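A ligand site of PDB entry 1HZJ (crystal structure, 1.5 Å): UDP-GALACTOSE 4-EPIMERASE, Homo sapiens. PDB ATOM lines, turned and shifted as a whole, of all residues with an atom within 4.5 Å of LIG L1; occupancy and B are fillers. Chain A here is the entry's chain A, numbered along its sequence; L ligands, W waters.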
ATOM      1  N   GLY A   9     -30.239  25.077   6.542  1.00  0.00           N
ATOM      2  CA  GLY A   9     -30.954  25.352   5.297  1.00  0.00           C
ATOM      3  C   GLY A   9     -32.288  24.562   5.233  1.00  0.00           C
ATOM      4  O   GLY A   9     -32.785  24.209   4.146  1.00  0.00           O
ATOM      5  N   ALA A  11     -35.368  25.455   5.635  1.00  0.00           N
ATOM      6  CA  ALA A  11     -36.568  26.124   5.078  1.00  0.00           C
ATOM      7  C   ALA A  11     -36.661  25.954   3.573  1.00  0.00           C
ATOM      8  O   ALA A  11     -37.682  26.274   2.963  1.00  0.00           O
ATOM      9  CB  ALA A  11     -36.597  27.612   5.461  1.00  0.00           C
ATOM     10  N   GLY A  12     -35.585  25.467   2.943  1.00  0.00           N
ATOM     11  CA  GLY A  12     -35.471  25.280   1.511  1.00  0.00           C
ATOM     12  C   GLY A  12     -36.249  24.112   0.941  1.00  0.00           C
ATOM     13  O   GLY A  12     -37.004  23.436   1.608  1.00  0.00           O
ATOM     14  N   TYR A  13     -36.054  23.873  -0.315  1.00  0.00           N
ATOM     15  CA  TYR A  13     -36.764  22.820  -0.996  1.00  0.00           C
ATOM     16  C   TYR A  13     -36.600  21.449  -0.409  1.00  0.00           C
ATOM     17  O   TYR A  13     -37.543  20.831   0.101  1.00  0.00           O
ATOM     18  CB  TYR A  13     -36.364  22.772  -2.457  1.00  0.00           C
ATOM     19  CG  TYR A  13     -37.013  21.706  -3.323  1.00  0.00           C
ATOM     20  CD1 TYR A  13     -38.337  21.264  -3.152  1.00  0.00           C
ATOM     21  CD2 TYR A  13     -36.280  21.157  -4.374  1.00  0.00           C
ATOM     22  CE1 TYR A  13     -38.880  20.288  -4.000  1.00  0.00           C
ATOM     23  CE2 TYR A  13     -36.809  20.197  -5.244  1.00  0.00           C
ATOM     24  CZ  TYR A  13     -38.115  19.742  -5.033  1.00  0.00           C
ATOM     25  OH  TYR A  13     -38.641  18.788  -5.849  1.00  0.00           O
ATOM     26  N   ILE A  14     -35.381  20.948  -0.505  1.00  0.00           N
ATOM     27  CA  ILE A  14     -35.122  19.601   0.035  1.00  0.00           C
ATOM     28  C   ILE A  14     -35.218  19.530   1.563  1.00  0.00           C
ATOM     29  O   ILE A  14     -35.733  18.570   2.132  1.00  0.00           O
ATOM     30  CB  ILE A  14     -33.766  19.015  -0.480  1.00  0.00           C
ATOM     31  CG1 ILE A  14     -33.700  19.100  -2.001  1.00  0.00           C
ATOM     32  CG2 ILE A  14     -33.631  17.558  -0.072  1.00  0.00           C
ATOM     33  CD1 ILE A  14     -32.345  18.726  -2.597  1.00  0.00           C
ATOM     34  N   GLY A  15     -34.720  20.548   2.214  1.00  0.00           N
ATOM     35  CA  GLY A  15     -34.738  20.591   3.642  1.00  0.00           C
ATOM     36  C   GLY A  15     -36.139  20.566   4.225  1.00  0.00           C
ATOM     37  O   GLY A  15     -36.385  19.891   5.216  1.00  0.00           O
ATOM     38  N   ASP A  33     -31.781  28.737   9.253  1.00  0.00           N
ATOM     39  CA  ASP A  33     -31.857  29.237   7.882  1.00  0.00           C
ATOM     40  C   ASP A  33     -31.708  30.759   7.900  1.00  0.00           C
ATOM     41  O   ASP A  33     -32.145  31.388   8.887  1.00  0.00           O
ATOM     42  CB  ASP A  33     -33.179  28.789   7.166  1.00  0.00           C
ATOM     43  CG  ASP A  33     -33.077  28.673   5.657  1.00  0.00           C
ATOM     44  OD1 ASP A  33     -33.177  27.614   5.062  1.00  0.00           O
ATOM     45  OD2 ASP A  33     -32.870  29.819   5.052  1.00  0.00           O
ATOM     46  N   ASN A  34     -31.095  31.307   6.844  1.00  0.00           N
ATOM     47  CA  ASN A  34     -30.921  32.747   6.769  1.00  0.00           C
ATOM     48  C   ASN A  34     -31.868  33.413   5.791  1.00  0.00           C
ATOM     49  O   ASN A  34     -31.710  34.595   5.521  1.00  0.00           O
ATOM     50  CB  ASN A  34     -29.479  33.159   6.429  1.00  0.00           C
ATOM     51  CG  ASN A  34     -29.060  32.834   5.016  1.00  0.00           C
ATOM     52  OD1 ASN A  34     -29.778  32.119   4.285  1.00  0.00           O
ATOM     53  ND2 ASN A  34     -27.890  33.322   4.622  1.00  0.00           N
ATOM     54  N   PHE A  35     -32.828  32.653   5.275  1.00  0.00           N
ATOM     55  CA  PHE A  35     -33.786  33.140   4.312  1.00  0.00           C
ATOM     56  C   PHE A  35     -33.184  33.572   2.987  1.00  0.00           C
ATOM     57  O   PHE A  35     -33.843  34.273   2.207  1.00  0.00           O
ATOM     58  CB  PHE A  35     -34.659  34.270   4.922  1.00  0.00           C
ATOM     59  CG  PHE A  35     -35.557  33.781   6.029  1.00  0.00           C
ATOM     60  CD1 PHE A  35     -35.287  34.046   7.366  1.00  0.00           C
ATOM     61  CD2 PHE A  35     -36.675  32.999   5.728  1.00  0.00           C
ATOM     62  CE1 PHE A  35     -36.138  33.597   8.373  1.00  0.00           C
ATOM     63  CE2 PHE A  35     -37.539  32.520   6.719  1.00  0.00           C
ATOM     64  CZ  PHE A  35     -37.255  32.829   8.052  1.00  0.00           C
ATOM     65  N   HIS A  36     -31.933  33.202   2.681  1.00  0.00           N
ATOM     66  CA  HIS A  36     -31.325  33.601   1.398  1.00  0.00           C
ATOM     67  C   HIS A  36     -32.166  33.141   0.222  1.00  0.00           C
ATOM     68  O   HIS A  36     -32.279  33.863  -0.776  1.00  0.00           O
ATOM     69  CB  HIS A  36     -29.898  33.052   1.206  1.00  0.00           C
ATOM     70  CG  HIS A  36     -29.434  33.161  -0.204  1.00  0.00           C
ATOM     71  ND1 HIS A  36     -28.938  34.369  -0.697  1.00  0.00           N
ATOM     72  CD2 HIS A  36     -29.377  32.243  -1.215  1.00  0.00           C
ATOM     73  CE1 HIS A  36     -28.606  34.157  -1.972  1.00  0.00           C
ATOM     74  NE2 HIS A  36     -28.860  32.906  -2.331  1.00  0.00           N
ATOM     75  N   ASN A  37     -32.744  31.941   0.344  1.00  0.00           N
ATOM     76  CA  ASN A  37     -33.564  31.361  -0.716  1.00  0.00           C
ATOM     77  C   ASN A  37     -34.834  30.710  -0.191  1.00  0.00           C
ATOM     78  O   ASN A  37     -35.228  29.647  -0.649  1.00  0.00           O
ATOM     79  CB  ASN A  37     -32.781  30.270  -1.493  1.00  0.00           C
ATOM     80  CG  ASN A  37     -33.391  30.029  -2.870  1.00  0.00           C
ATOM     81  OD1 ASN A  37     -33.941  30.943  -3.508  1.00  0.00           O
ATOM     82  ND2 ASN A  37     -33.272  28.826  -3.399  1.00  0.00           N
ATOM     83  N   ALA A  38     -35.464  31.346   0.786  1.00  0.00           N
ATOM     84  CA  ALA A  38     -36.683  30.814   1.376  1.00  0.00           C
ATOM     85  C   ALA A  38     -37.539  31.985   1.772  1.00  0.00           C
ATOM     86  O   ALA A  38     -37.066  32.975   2.314  1.00  0.00           O
ATOM     87  CB  ALA A  38     -36.401  30.004   2.633  1.00  0.00           C
ATOM     88  N   MET A  65     -30.570  32.322  11.230  1.00  0.00           N
ATOM     89  CA  MET A  65     -29.145  32.574  11.411  1.00  0.00           C
ATOM     90  C   MET A  65     -28.361  32.117  10.217  1.00  0.00           C
ATOM     91  O   MET A  65     -28.889  31.346   9.397  1.00  0.00           O
ATOM     92  CB  MET A  65     -28.555  32.017  12.708  1.00  0.00           C
ATOM     93  CG  MET A  65     -28.424  30.505  12.716  1.00  0.00           C
ATOM     94  SD  MET A  65     -27.441  29.851  14.105  1.00  0.00           S
ATOM     95  CE  MET A  65     -25.852  29.861  13.243  1.00  0.00           C
ATOM     96  N   ASP A  66     -27.113  32.623  10.121  1.00  0.00           N
ATOM     97  CA  ASP A  66     -26.206  32.312   9.050  1.00  0.00           C
ATOM     98  C   ASP A  66     -25.109  31.343   9.528  1.00  0.00           C
ATOM     99  O   ASP A  66     -24.592  31.463  10.624  1.00  0.00           O
ATOM    100  CB  ASP A  66     -25.592  33.611   8.526  1.00  0.00           C
ATOM    101  CG  ASP A  66     -25.037  33.409   7.130  1.00  0.00           C
ATOM    102  OD1 ASP A  66     -24.297  32.497   6.847  1.00  0.00           O
ATOM    103  OD2 ASP A  66     -25.444  34.286   6.255  1.00  0.00           O
ATOM    104  N   ILE A  67     -24.818  30.336   8.701  1.00  0.00           N
ATOM    105  CA  ILE A  67     -23.792  29.361   9.073  1.00  0.00           C
ATOM    106  C   ILE A  67     -22.449  30.053   9.066  1.00  0.00           C
ATOM    107  O   ILE A  67     -21.495  29.483   9.564  1.00  0.00           O
ATOM    108  CB  ILE A  67     -23.725  28.143   8.148  1.00  0.00           C
ATOM    109  CG1 ILE A  67     -23.369  28.577   6.729  1.00  0.00           C
ATOM    110  CG2 ILE A  67     -24.953  27.221   8.212  1.00  0.00           C
ATOM    111  CD1 ILE A  67     -23.216  27.433   5.716  1.00  0.00           C
ATOM    112  N   PHE A  88     -28.003  21.105   4.643  1.00  0.00           N
ATOM    113  CA  PHE A  88     -28.478  21.528   3.333  1.00  0.00           C
ATOM    114  C   PHE A  88     -28.088  22.962   2.936  1.00  0.00           C
ATOM    115  O   PHE A  88     -28.107  23.288   1.746  1.00  0.00           O
ATOM    116  CB  PHE A  88     -30.024  21.560   3.298  1.00  0.00           C
ATOM    117  CG  PHE A  88     -30.700  20.224   3.511  1.00  0.00           C
ATOM    118  CD1 PHE A  88     -30.779  19.301   2.470  1.00  0.00           C
ATOM    119  CD2 PHE A  88     -31.243  19.931   4.770  1.00  0.00           C
ATOM    120  CE1 PHE A  88     -31.397  18.049   2.639  1.00  0.00           C
ATOM    121  CE2 PHE A  88     -31.867  18.699   4.963  1.00  0.00           C
ATOM    122  CZ  PHE A  88     -31.963  17.794   3.888  1.00  0.00           C
ATOM    123  N   ALA A  89     -27.763  23.803   3.933  1.00  0.00           N
ATOM    124  CA  ALA A  89     -27.444  25.209   3.712  1.00  0.00           C
ATOM    125  C   ALA A  89     -26.322  25.429   2.699  1.00  0.00           C
ATOM    126  O   ALA A  89     -25.241  24.824   2.738  1.00  0.00           O
ATOM    127  CB  ALA A  89     -27.177  25.935   5.018  1.00  0.00           C
ATOM    128  N   GLY A  90     -26.576  26.314   1.793  1.00  0.00           N
ATOM    129  CA  GLY A  90     -25.601  26.657   0.802  1.00  0.00           C
ATOM    130  C   GLY A  90     -26.193  27.375  -0.405  1.00  0.00           C
ATOM    131  O   GLY A  90     -27.426  27.523  -0.493  1.00  0.00           O
ATOM    132  N   LEU A  91     -25.287  27.809  -1.291  1.00  0.00           N
ATOM    133  CA  LEU A  91     -25.668  28.450  -2.531  1.00  0.00           C
ATOM    134  C   LEU A  91     -25.622  27.365  -3.592  1.00  0.00           C
ATOM    135  O   LEU A  91     -24.740  26.508  -3.559  1.00  0.00           O
ATOM    136  CB  LEU A  91     -24.743  29.633  -2.910  1.00  0.00           C
ATOM    137  CG  LEU A  91     -24.544  30.700  -1.838  1.00  0.00           C
ATOM    138  CD1 LEU A  91     -23.729  31.875  -2.412  1.00  0.00           C
ATOM    139  CD2 LEU A  91     -25.904  31.215  -1.373  1.00  0.00           C
ATOM    140  N   LYS A  92     -26.545  27.366  -4.570  1.00  0.00           N
ATOM    141  CA  LYS A  92     -26.559  26.326  -5.570  1.00  0.00           C
ATOM    142  C   LYS A  92     -26.824  26.734  -7.008  1.00  0.00           C
ATOM    143  O   LYS A  92     -27.042  25.831  -7.814  1.00  0.00           O
ATOM    144  CB  LYS A  92     -27.583  25.261  -5.183  1.00  0.00           C
ATOM    145  CG  LYS A  92     -29.024  25.818  -5.204  1.00  0.00           C
ATOM    146  CD  LYS A  92     -30.124  24.739  -5.257  1.00  0.00           C
ATOM    147  CE  LYS A  92     -31.516  25.389  -5.316  1.00  0.00           C
ATOM    148  NZ  LYS A  92     -32.617  24.468  -5.722  1.00  0.00           N
ATOM    149  N   VAL A 107     -19.687  31.052   1.057  1.00  0.00           N
ATOM    150  CA  VAL A 107     -20.820  30.394   1.678  1.00  0.00           C
ATOM    151  C   VAL A 107     -20.683  28.892   1.832  1.00  0.00           C
ATOM    152  O   VAL A 107     -20.886  28.305   2.895  1.00  0.00           O
ATOM    153  CB  VAL A 107     -22.122  30.725   0.948  1.00  0.00           C
ATOM    154  CG1 VAL A 107     -23.256  30.032   1.685  1.00  0.00           C
ATOM    155  CG2 VAL A 107     -22.334  32.242   0.945  1.00  0.00           C
ATOM    156  N   SER A 130     -25.413  17.222   2.130  1.00  0.00           N
ATOM    157  CA  SER A 130     -26.046  17.355   0.845  1.00  0.00           C
ATOM    158  C   SER A 130     -25.048  17.461  -0.262  1.00  0.00           C
ATOM    159  O   SER A 130     -24.601  18.551  -0.586  1.00  0.00           O
ATOM    160  CB  SER A 130     -26.959  18.585   0.743  1.00  0.00           C
ATOM    161  OG  SER A 130     -27.938  18.556   1.756  1.00  0.00           O
ATOM    162  N   SER A 131     -24.698  16.368  -0.903  1.00  0.00           N
ATOM    163  CA  SER A 131     -23.778  16.457  -2.016  1.00  0.00           C
ATOM    164  C   SER A 131     -24.556  16.356  -3.345  1.00  0.00           C
ATOM    165  O   SER A 131     -25.782  16.468  -3.354  1.00  0.00           O
ATOM    166  CB  SER A 131     -22.657  15.434  -1.906  1.00  0.00           C
ATOM    167  OG  SER A 131     -21.688  15.728  -2.890  1.00  0.00           O
ATOM    168  N   SER A 132     -23.878  16.098  -4.461  1.00  0.00           N
ATOM    169  CA  SER A 132     -24.601  16.026  -5.707  1.00  0.00           C
ATOM    170  C   SER A 132     -23.851  15.225  -6.737  1.00  0.00           C
ATOM    171  O   SER A 132     -22.622  15.187  -6.762  1.00  0.00           O
ATOM    172  CB  SER A 132     -24.646  17.496  -6.166  1.00  0.00           C
ATOM    173  OG  SER A 132     -24.888  17.610  -7.558  1.00  0.00           O
ATOM    174  N   TYR A 157     -19.645  26.094  -8.376  1.00  0.00           N
ATOM    175  CA  TYR A 157     -20.618  25.397  -7.536  1.00  0.00           C
ATOM    176  C   TYR A 157     -20.232  23.935  -7.302  1.00  0.00           C
ATOM    177  O   TYR A 157     -20.122  23.476  -6.170  1.00  0.00           O
ATOM    178  CB  TYR A 157     -22.048  25.442  -8.117  1.00  0.00           C
ATOM    179  CG  TYR A 157     -22.994  24.463  -7.414  1.00  0.00           C
ATOM    180  CD1 TYR A 157     -23.478  23.332  -8.092  1.00  0.00           C
ATOM    181  CD2 TYR A 157     -23.372  24.657  -6.089  1.00  0.00           C
ATOM    182  CE1 TYR A 157     -24.340  22.437  -7.447  1.00  0.00           C
ATOM    183  CE2 TYR A 157     -24.242  23.771  -5.437  1.00  0.00           C
ATOM    184  CZ  TYR A 157     -24.721  22.647  -6.121  1.00  0.00           C
ATOM    185  OH  TYR A 157     -25.582  21.761  -5.504  1.00  0.00           O
ATOM    186  N   LYS A 161     -18.724  21.615  -3.884  1.00  0.00           N
ATOM    187  CA  LYS A 161     -19.298  20.378  -3.330  1.00  0.00           C
ATOM    188  C   LYS A 161     -18.220  19.300  -3.265  1.00  0.00           C
ATOM    189  O   LYS A 161     -18.140  18.535  -2.285  1.00  0.00           O
ATOM    190  CB  LYS A 161     -20.484  19.887  -4.174  1.00  0.00           C
ATOM    191  CG  LYS A 161     -21.770  20.720  -3.908  1.00  0.00           C
ATOM    192  CD  LYS A 161     -22.315  20.643  -2.475  1.00  0.00           C
ATOM    193  CE  LYS A 161     -23.683  21.286  -2.309  1.00  0.00           C
ATOM    194  NZ  LYS A 161     -24.169  21.257  -0.910  1.00  0.00           N
ATOM    195  N   TYR A 185     -27.090  13.601  -4.430  1.00  0.00           N
ATOM    196  CA  TYR A 185     -28.392  13.627  -5.047  1.00  0.00           C
ATOM    197  C   TYR A 185     -28.264  13.729  -6.538  1.00  0.00           C
ATOM    198  O   TYR A 185     -27.335  14.395  -7.075  1.00  0.00           O
ATOM    199  CB  TYR A 185     -29.168  14.911  -4.668  1.00  0.00           C
ATOM    200  CG  TYR A 185     -29.205  15.302  -3.226  1.00  0.00           C
ATOM    201  CD1 TYR A 185     -29.108  14.358  -2.199  1.00  0.00           C
ATOM    202  CD2 TYR A 185     -29.373  16.637  -2.865  1.00  0.00           C
ATOM    203  CE1 TYR A 185     -29.145  14.729  -0.849  1.00  0.00           C
ATOM    204  CE2 TYR A 185     -29.454  17.032  -1.526  1.00  0.00           C
ATOM    205  CZ  TYR A 185     -29.335  16.076  -0.517  1.00  0.00           C
ATOM    206  OH  TYR A 185     -29.362  16.469   0.795  1.00  0.00           O
ATOM    207  N   PHE A 186     -29.237  13.088  -7.207  1.00  0.00           N
ATOM    208  CA  PHE A 186     -29.289  13.188  -8.644  1.00  0.00           C
ATOM    209  C   PHE A 186     -30.201  14.399  -8.981  1.00  0.00           C
ATOM    210  O   PHE A 186     -29.828  15.505  -8.628  1.00  0.00           O
ATOM    211  CB  PHE A 186     -29.609  11.887  -9.376  1.00  0.00           C
ATOM    212  CG  PHE A 186     -28.305  11.108  -9.500  1.00  0.00           C
ATOM    213  CD1 PHE A 186     -27.684  10.929 -10.729  1.00  0.00           C
ATOM    214  CD2 PHE A 186     -27.687  10.594  -8.360  1.00  0.00           C
ATOM    215  CE1 PHE A 186     -26.463  10.240 -10.829  1.00  0.00           C
ATOM    216  CE2 PHE A 186     -26.469   9.914  -8.430  1.00  0.00           C
ATOM    217  CZ  PHE A 186     -25.856   9.753  -9.681  1.00  0.00           C
ATOM    218  N   PRO A 188     -33.527  16.051  -8.029  1.00  0.00           N
ATOM    219  CA  PRO A 188     -34.679  16.121  -7.141  1.00  0.00           C
ATOM    220  C   PRO A 188     -35.859  16.798  -7.810  1.00  0.00           C
ATOM    221  O   PRO A 188     -35.736  17.888  -8.443  1.00  0.00           O
ATOM    222  CB  PRO A 188     -34.224  16.894  -5.916  1.00  0.00           C
ATOM    223  CG  PRO A 188     -32.698  16.951  -5.980  1.00  0.00           C
ATOM    224  CD  PRO A 188     -32.341  16.762  -7.446  1.00  0.00           C
HETATM  225  P1  LIG L   1     -32.541  25.594  -1.406  1.00  0.00           P
HETATM  226  O1  LIG L   1     -34.029  25.561  -1.537  1.00  0.00           O
HETATM  227  O2  LIG L   1     -31.933  26.859  -1.840  1.00  0.00           O
HETATM  228  O3  LIG L   1     -32.260  25.355   0.115  1.00  0.00           O
HETATM  229  C1  LIG L   1     -31.044  25.803   0.737  1.00  0.00           C
HETATM  230  C2  LIG L   1     -31.411  26.554   1.960  1.00  0.00           C
HETATM  231  O4  LIG L   1     -30.189  27.113   2.525  1.00  0.00           O
HETATM  232  C3  LIG L   1     -32.314  27.771   1.641  1.00  0.00           C
HETATM  233  O5  LIG L   1     -33.500  27.716   2.432  1.00  0.00           O
HETATM  234  C4  LIG L   1     -31.370  28.958   1.960  1.00  0.00           C
HETATM  235  O6  LIG L   1     -32.018  30.158   2.436  1.00  0.00           O
HETATM  236  C5  LIG L   1     -30.450  28.385   3.025  1.00  0.00           C
HETATM  237  N1  LIG L   1     -29.168  29.080   3.081  1.00  0.00           N
HETATM  238  C6  LIG L   1     -28.364  29.519   2.049  1.00  0.00           C
HETATM  239  N2  LIG L   1     -27.229  30.096   2.483  1.00  0.00           N
HETATM  240  C7  LIG L   1     -27.319  29.992   3.866  1.00  0.00           C
HETATM  241  C8  LIG L   1     -26.439  30.396   4.897  1.00  0.00           C
HETATM  242  N3  LIG L   1     -25.260  31.030   4.707  1.00  0.00           N
HETATM  243  N4  LIG L   1     -26.836  30.154   6.159  1.00  0.00           N
HETATM  244  C9  LIG L   1     -28.051  29.539   6.399  1.00  0.00           C
HETATM  245  N5  LIG L   1     -28.931  29.143   5.527  1.00  0.00           N
HETATM  246  C10 LIG L   1     -28.514  29.400   4.267  1.00  0.00           C
HETATM  247  O7  LIG L   1     -31.912  24.424  -2.215  1.00  0.00           O
HETATM  248  P2  LIG L   1     -32.267  22.848  -2.286  1.00  0.00           P
HETATM  249  O8  LIG L   1     -32.727  22.495  -3.623  1.00  0.00           O
HETATM  250  O9  LIG L   1     -33.147  22.542  -1.116  1.00  0.00           O
HETATM  251  O10 LIG L   1     -30.827  22.139  -2.032  1.00  0.00           O
HETATM  252  C11 LIG L   1     -30.478  21.712  -0.697  1.00  0.00           C
HETATM  253  C12 LIG L   1     -29.007  21.357  -0.764  1.00  0.00           C
HETATM  254  O11 LIG L   1     -28.899  20.274  -1.692  1.00  0.00           O
HETATM  255  C13 LIG L   1     -27.997  22.445  -1.235  1.00  0.00           C
HETATM  256  O12 LIG L   1     -26.749  22.393  -0.503  1.00  0.00           O
HETATM  257  C14 LIG L   1     -27.804  22.050  -2.702  1.00  0.00           C
HETATM  258  O13 LIG L   1     -26.518  22.542  -3.133  1.00  0.00           O
HETATM  259  C15 LIG L   1     -27.906  20.535  -2.659  1.00  0.00           C
HETATM  260  N6  LIG L   1     -28.284  19.896  -3.936  1.00  0.00           N
HETATM  261  C16 LIG L   1     -29.458  20.317  -4.498  1.00  0.00           C
HETATM  262  C17 LIG L   1     -29.815  19.868  -5.763  1.00  0.00           C
HETATM  263  C18 LIG L   1     -31.155  20.313  -6.406  1.00  0.00           C
HETATM  264  O14 LIG L   1     -31.438  19.962  -7.550  1.00  0.00           O
HETATM  265  N7  LIG L   1     -32.045  21.038  -5.703  1.00  0.00           N
HETATM  266  C19 LIG L   1     -29.049  18.839  -6.423  1.00  0.00           C
HETATM  267  C20 LIG L   1     -27.946  18.412  -5.675  1.00  0.00           C
HETATM  268  C21 LIG L   1     -27.490  18.883  -4.480  1.00  0.00           C
HETATM  269  C1  LG2 L   2     -28.303  20.923 -13.136  1.00  0.00           C
HETATM  270  C2  LG2 L   2     -27.070  21.665 -12.623  1.00  0.00           C
HETATM  271  C3  LG2 L   2     -26.341  20.840 -11.553  1.00  0.00           C
HETATM  272  C4  LG2 L   2     -27.299  20.412 -10.442  1.00  0.00           C
HETATM  273  C5  LG2 L   2     -28.466  19.642 -11.050  1.00  0.00           C
HETATM  274  C6  LG2 L   2     -29.580  19.453 -10.045  1.00  0.00           C
HETATM  275  C7  LG2 L   2     -26.308  22.978 -14.494  1.00  0.00           C
HETATM  276  C8  LG2 L   2     -25.329  23.308 -15.582  1.00  0.00           C
HETATM  277  N1  LG2 L   2     -26.097  21.900 -13.713  1.00  0.00           N
HETATM  278  O1  LG2 L   2     -27.891  19.809 -13.887  1.00  0.00           O
HETATM  279  O2  LG2 L   2     -25.328  21.646 -10.952  1.00  0.00           O
HETATM  280  O3  LG2 L   2     -26.659  19.642  -9.407  1.00  0.00           O
HETATM  281  O4  LG2 L   2     -29.107  20.467 -12.047  1.00  0.00           O
HETATM  282  O5  LG2 L   2     -29.965  20.767  -9.616  1.00  0.00           O
HETATM  283  O6  LG2 L   2     -27.292  23.673 -14.338  1.00  0.00           O
HETATM  284  N2  LG2 L   2     -33.138  21.600 -19.756  1.00  0.00           N
HETATM  285  C9  LG2 L   2     -33.769  22.117 -20.885  1.00  0.00           C
HETATM  286  N3  LG2 L   2     -34.398  23.303 -20.660  1.00  0.00           N
HETATM  287  C10 LG2 L   2     -34.475  24.004 -19.447  1.00  0.00           C
HETATM  288  C11 LG2 L   2     -33.782  23.372 -18.360  1.00  0.00           C
HETATM  289  C12 LG2 L   2     -33.148  22.253 -18.543  1.00  0.00           C
HETATM  290  O7  LG2 L   2     -33.777  21.549 -21.971  1.00  0.00           O
HETATM  291  O8  LG2 L   2     -35.086  25.041 -19.404  1.00  0.00           O
HETATM  292  C13 LG2 L   2     -32.479  20.284 -19.870  1.00  0.00           C
HETATM  293  C14 LG2 L   2     -31.018  20.270 -19.544  1.00  0.00           C
HETATM  294  O9  LG2 L   2     -30.255  20.460 -20.739  1.00  0.00           O
HETATM  295  C15 LG2 L   2     -30.844  18.786 -19.113  1.00  0.00           C
HETATM  296  C16 LG2 L   2     -32.140  18.497 -18.370  1.00  0.00           C
HETATM  297  O10 LG2 L   2     -33.092  19.447 -18.909  1.00  0.00           O
HETATM  298  O11 LG2 L   2     -30.661  17.890 -20.207  1.00  0.00           O
HETATM  299  C17 LG2 L   2     -32.125  18.655 -16.862  1.00  0.00           C
HETATM  300  O12 LG2 L   2     -31.641  19.961 -16.594  1.00  0.00           O
HETATM  301  P1  LG2 L   2     -31.457  20.519 -15.144  1.00  0.00           P
HETATM  302  O13 LG2 L   2     -30.853  21.881 -15.143  1.00  0.00           O
HETATM  303  O14 LG2 L   2     -32.693  20.498 -14.357  1.00  0.00           O
HETATM  304  O15 LG2 L   2     -30.442  19.438 -14.438  1.00  0.00           O
HETATM  305  P2  LG2 L   2     -28.962  19.036 -14.795  1.00  0.00           P
HETATM  306  O16 LG2 L   2     -28.923  17.569 -14.548  1.00  0.00           O
HETATM  307  O17 LG2 L   2     -28.684  19.270 -16.262  1.00  0.00           O
HETATM  308  O   HOH W   1     -25.109  21.953   1.959  1.00  0.00           O
HETATM  309  O   HOH W   2     -24.915  24.471  -1.730  1.00  0.00           O
HETATM  310  O   HOH W   3     -33.227  22.816   1.678  1.00  0.00           O
HETATM  311  O   HOH W   4     -27.377  16.750  -8.582  1.00  0.00           O
HETATM  312  O   HOH W   5     -33.565  19.304  -9.304  1.00  0.00           O
HETATM  313  O   HOH W   6     -24.547  34.165   3.736  1.00  0.00           O
HETATM  314  O   HOH W   7     -26.267  32.732   1.940  1.00  0.00           O
HETATM  315  O   HOH W   8     -29.568  28.540  -1.825  1.00  0.00           O
HETATM  316  O   HOH W   9     -34.027  22.344  -7.646  1.00  0.00           O
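The backbone carbonyl oxygen (O) of Phe 88 sits at hydrogen-bond distance from an oxygen (O12) of LIG L1.
NZ of Lys 161 is in hydrogen-bond range of O12 of LIG L1 (2.8 Å).
OG of Ser 132 is in hydrogen-bond range of O3 of LG2 L2, at 3.3 Å.
N of Ile 67 lies within hydrogen-bond range of N4 of LIG L1 (3.3 Å).
The backbone NH (N) of Ile 14 lies within hydrogen-bond range of an oxygen (O9) of LIG L1 (2.8 Å).
N5 of LIG L1 lies close to OD1 of Asn 34 (3.3 Å).
O1 of LIG L1 lies within hydrogen-bond range of N of Tyr 13, at 2.9 Å.
The side-chain amino group (NZ) of Lys 92 is in salt-bridge range of an oxygen (O8) of LIG L1, at 2.9 Å.
The side-chain carboxylate (OD1) of Asp 33 is in hydrogen-bond range of an oxygen (O5) of LIG L1 (2.7 Å).
An oxygen (O6) of LIG L1 is in hydrogen-bond range of the backbone NH (N) of Asn 37 (2.8 Å).
A nitrogen (N5) of LIG L1 is in hydrogen-bond range of the backbone NH (N) of Asn 34 (3.3 Å).
N of Gly 12 lies within hydrogen-bond range of O5 of LIG L1 (3.1 Å).
O6 of LIG L1 is in hydrogen-bond range of N of His 36.
The side-chain carboxylate of Asp 66 lies within hydrogen-bond range of a nitrogen (N3) of LIG L1 (2.8 Å).
OH of Tyr 157 lies within hydrogen-bond range of O13 of LIG L1, at 2.7 Å.
ND2 of Asn 37 sits at hydrogen-bond distance from O2 of LIG L1, at 2.8 Å.
An oxygen (O14) of LIG L1 sits at hydrogen-bond distance from an oxygen (O5) of LG2 L2 (2.7 Å).
N of Asn 34 sits at hydrogen-bond distance from O of Met 65 (3.4 Å).
The backbone carbonyl oxygen (O) of Ser 130 is in hydrogen-bond range of the side-chain amino group (NZ) of Lys 161, at 2.8 Å.
N of Met 65 is in hydrogen-bond range of O of Asp 33, 3.0 Å away.
OH of Tyr 185 lies within hydrogen-bond range of OG of Ser 130 (2.7 Å).
N of Ala 11 is in hydrogen-bond range of OD1 of Asp 33.
The side-chain carboxylate (OD2) of Asp 33 lies within hydrogen-bond range of the backbone NH (N) of Phe 35, at 2.8 Å.
The backbone carbonyl oxygen (O) of Ser 131 sits at hydrogen-bond distance from the backbone NH (N) of Tyr 185 (3.3 Å).
The side-chain carboxylate (OD2) of Asp 66 sits at hydrogen-bond distance from the side-chain amide nitrogen (ND2) of Asn 34, 3.1 Å away.
Residues that only touch LIG L1: Gly 9 (3.4 Å), Ala 11 (3.8 Å), Phe 35 (3.6 Å), Ala 38 (3.7 Å), Met 65 (3.6 Å), Ala 89 (3.5 Å), Gly 90 (3.4 Å), Val 107 (3.8 Å), Ser 130 (3.5 Å), Ser 131 (3.2 Å), Ser 132 (3.5 Å), Tyr 185 (3.3 Å) and Pro 188 (3.3 Å).
Of the 29 residues printed, 26 come within 4 Å of LIG L1.
The nearest printed residue that does not touch LIG L1 is Phe 186 (4.1 Å).
Water W7 bridges N2 of LIG L1 (2.9 Å) and ND2 of Asn 34 (3.2 Å).
Water W2 lies within hydrogen-bond range of the backbone carbonyl oxygen of Leu 91, an oxygen (O13) of LIG L1 and the side-chain amino group of Lys 161.
Water W8 lies within hydrogen-bond range of the backbone carbonyl oxygen (O) of Gly 90 and an oxygen (O2) of LIG L1.
Water W9 bridges N7 of LIG L1 (3.1 Å) and NZ of Lys 92 (3.2 Å).
Water W6 bridges the side-chain carboxylate (OD2) of Asp 66 (2.7 Å) and a nitrogen (N3) of LIG L1 (3.4 Å).
Water W4 lies within hydrogen-bond range of O of Phe 186 (2.7 Å), O of Tyr 185 (2.8 Å), OG of Ser 132 (2.8 Å) and O3 of LG2 L2 (3.1 Å).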
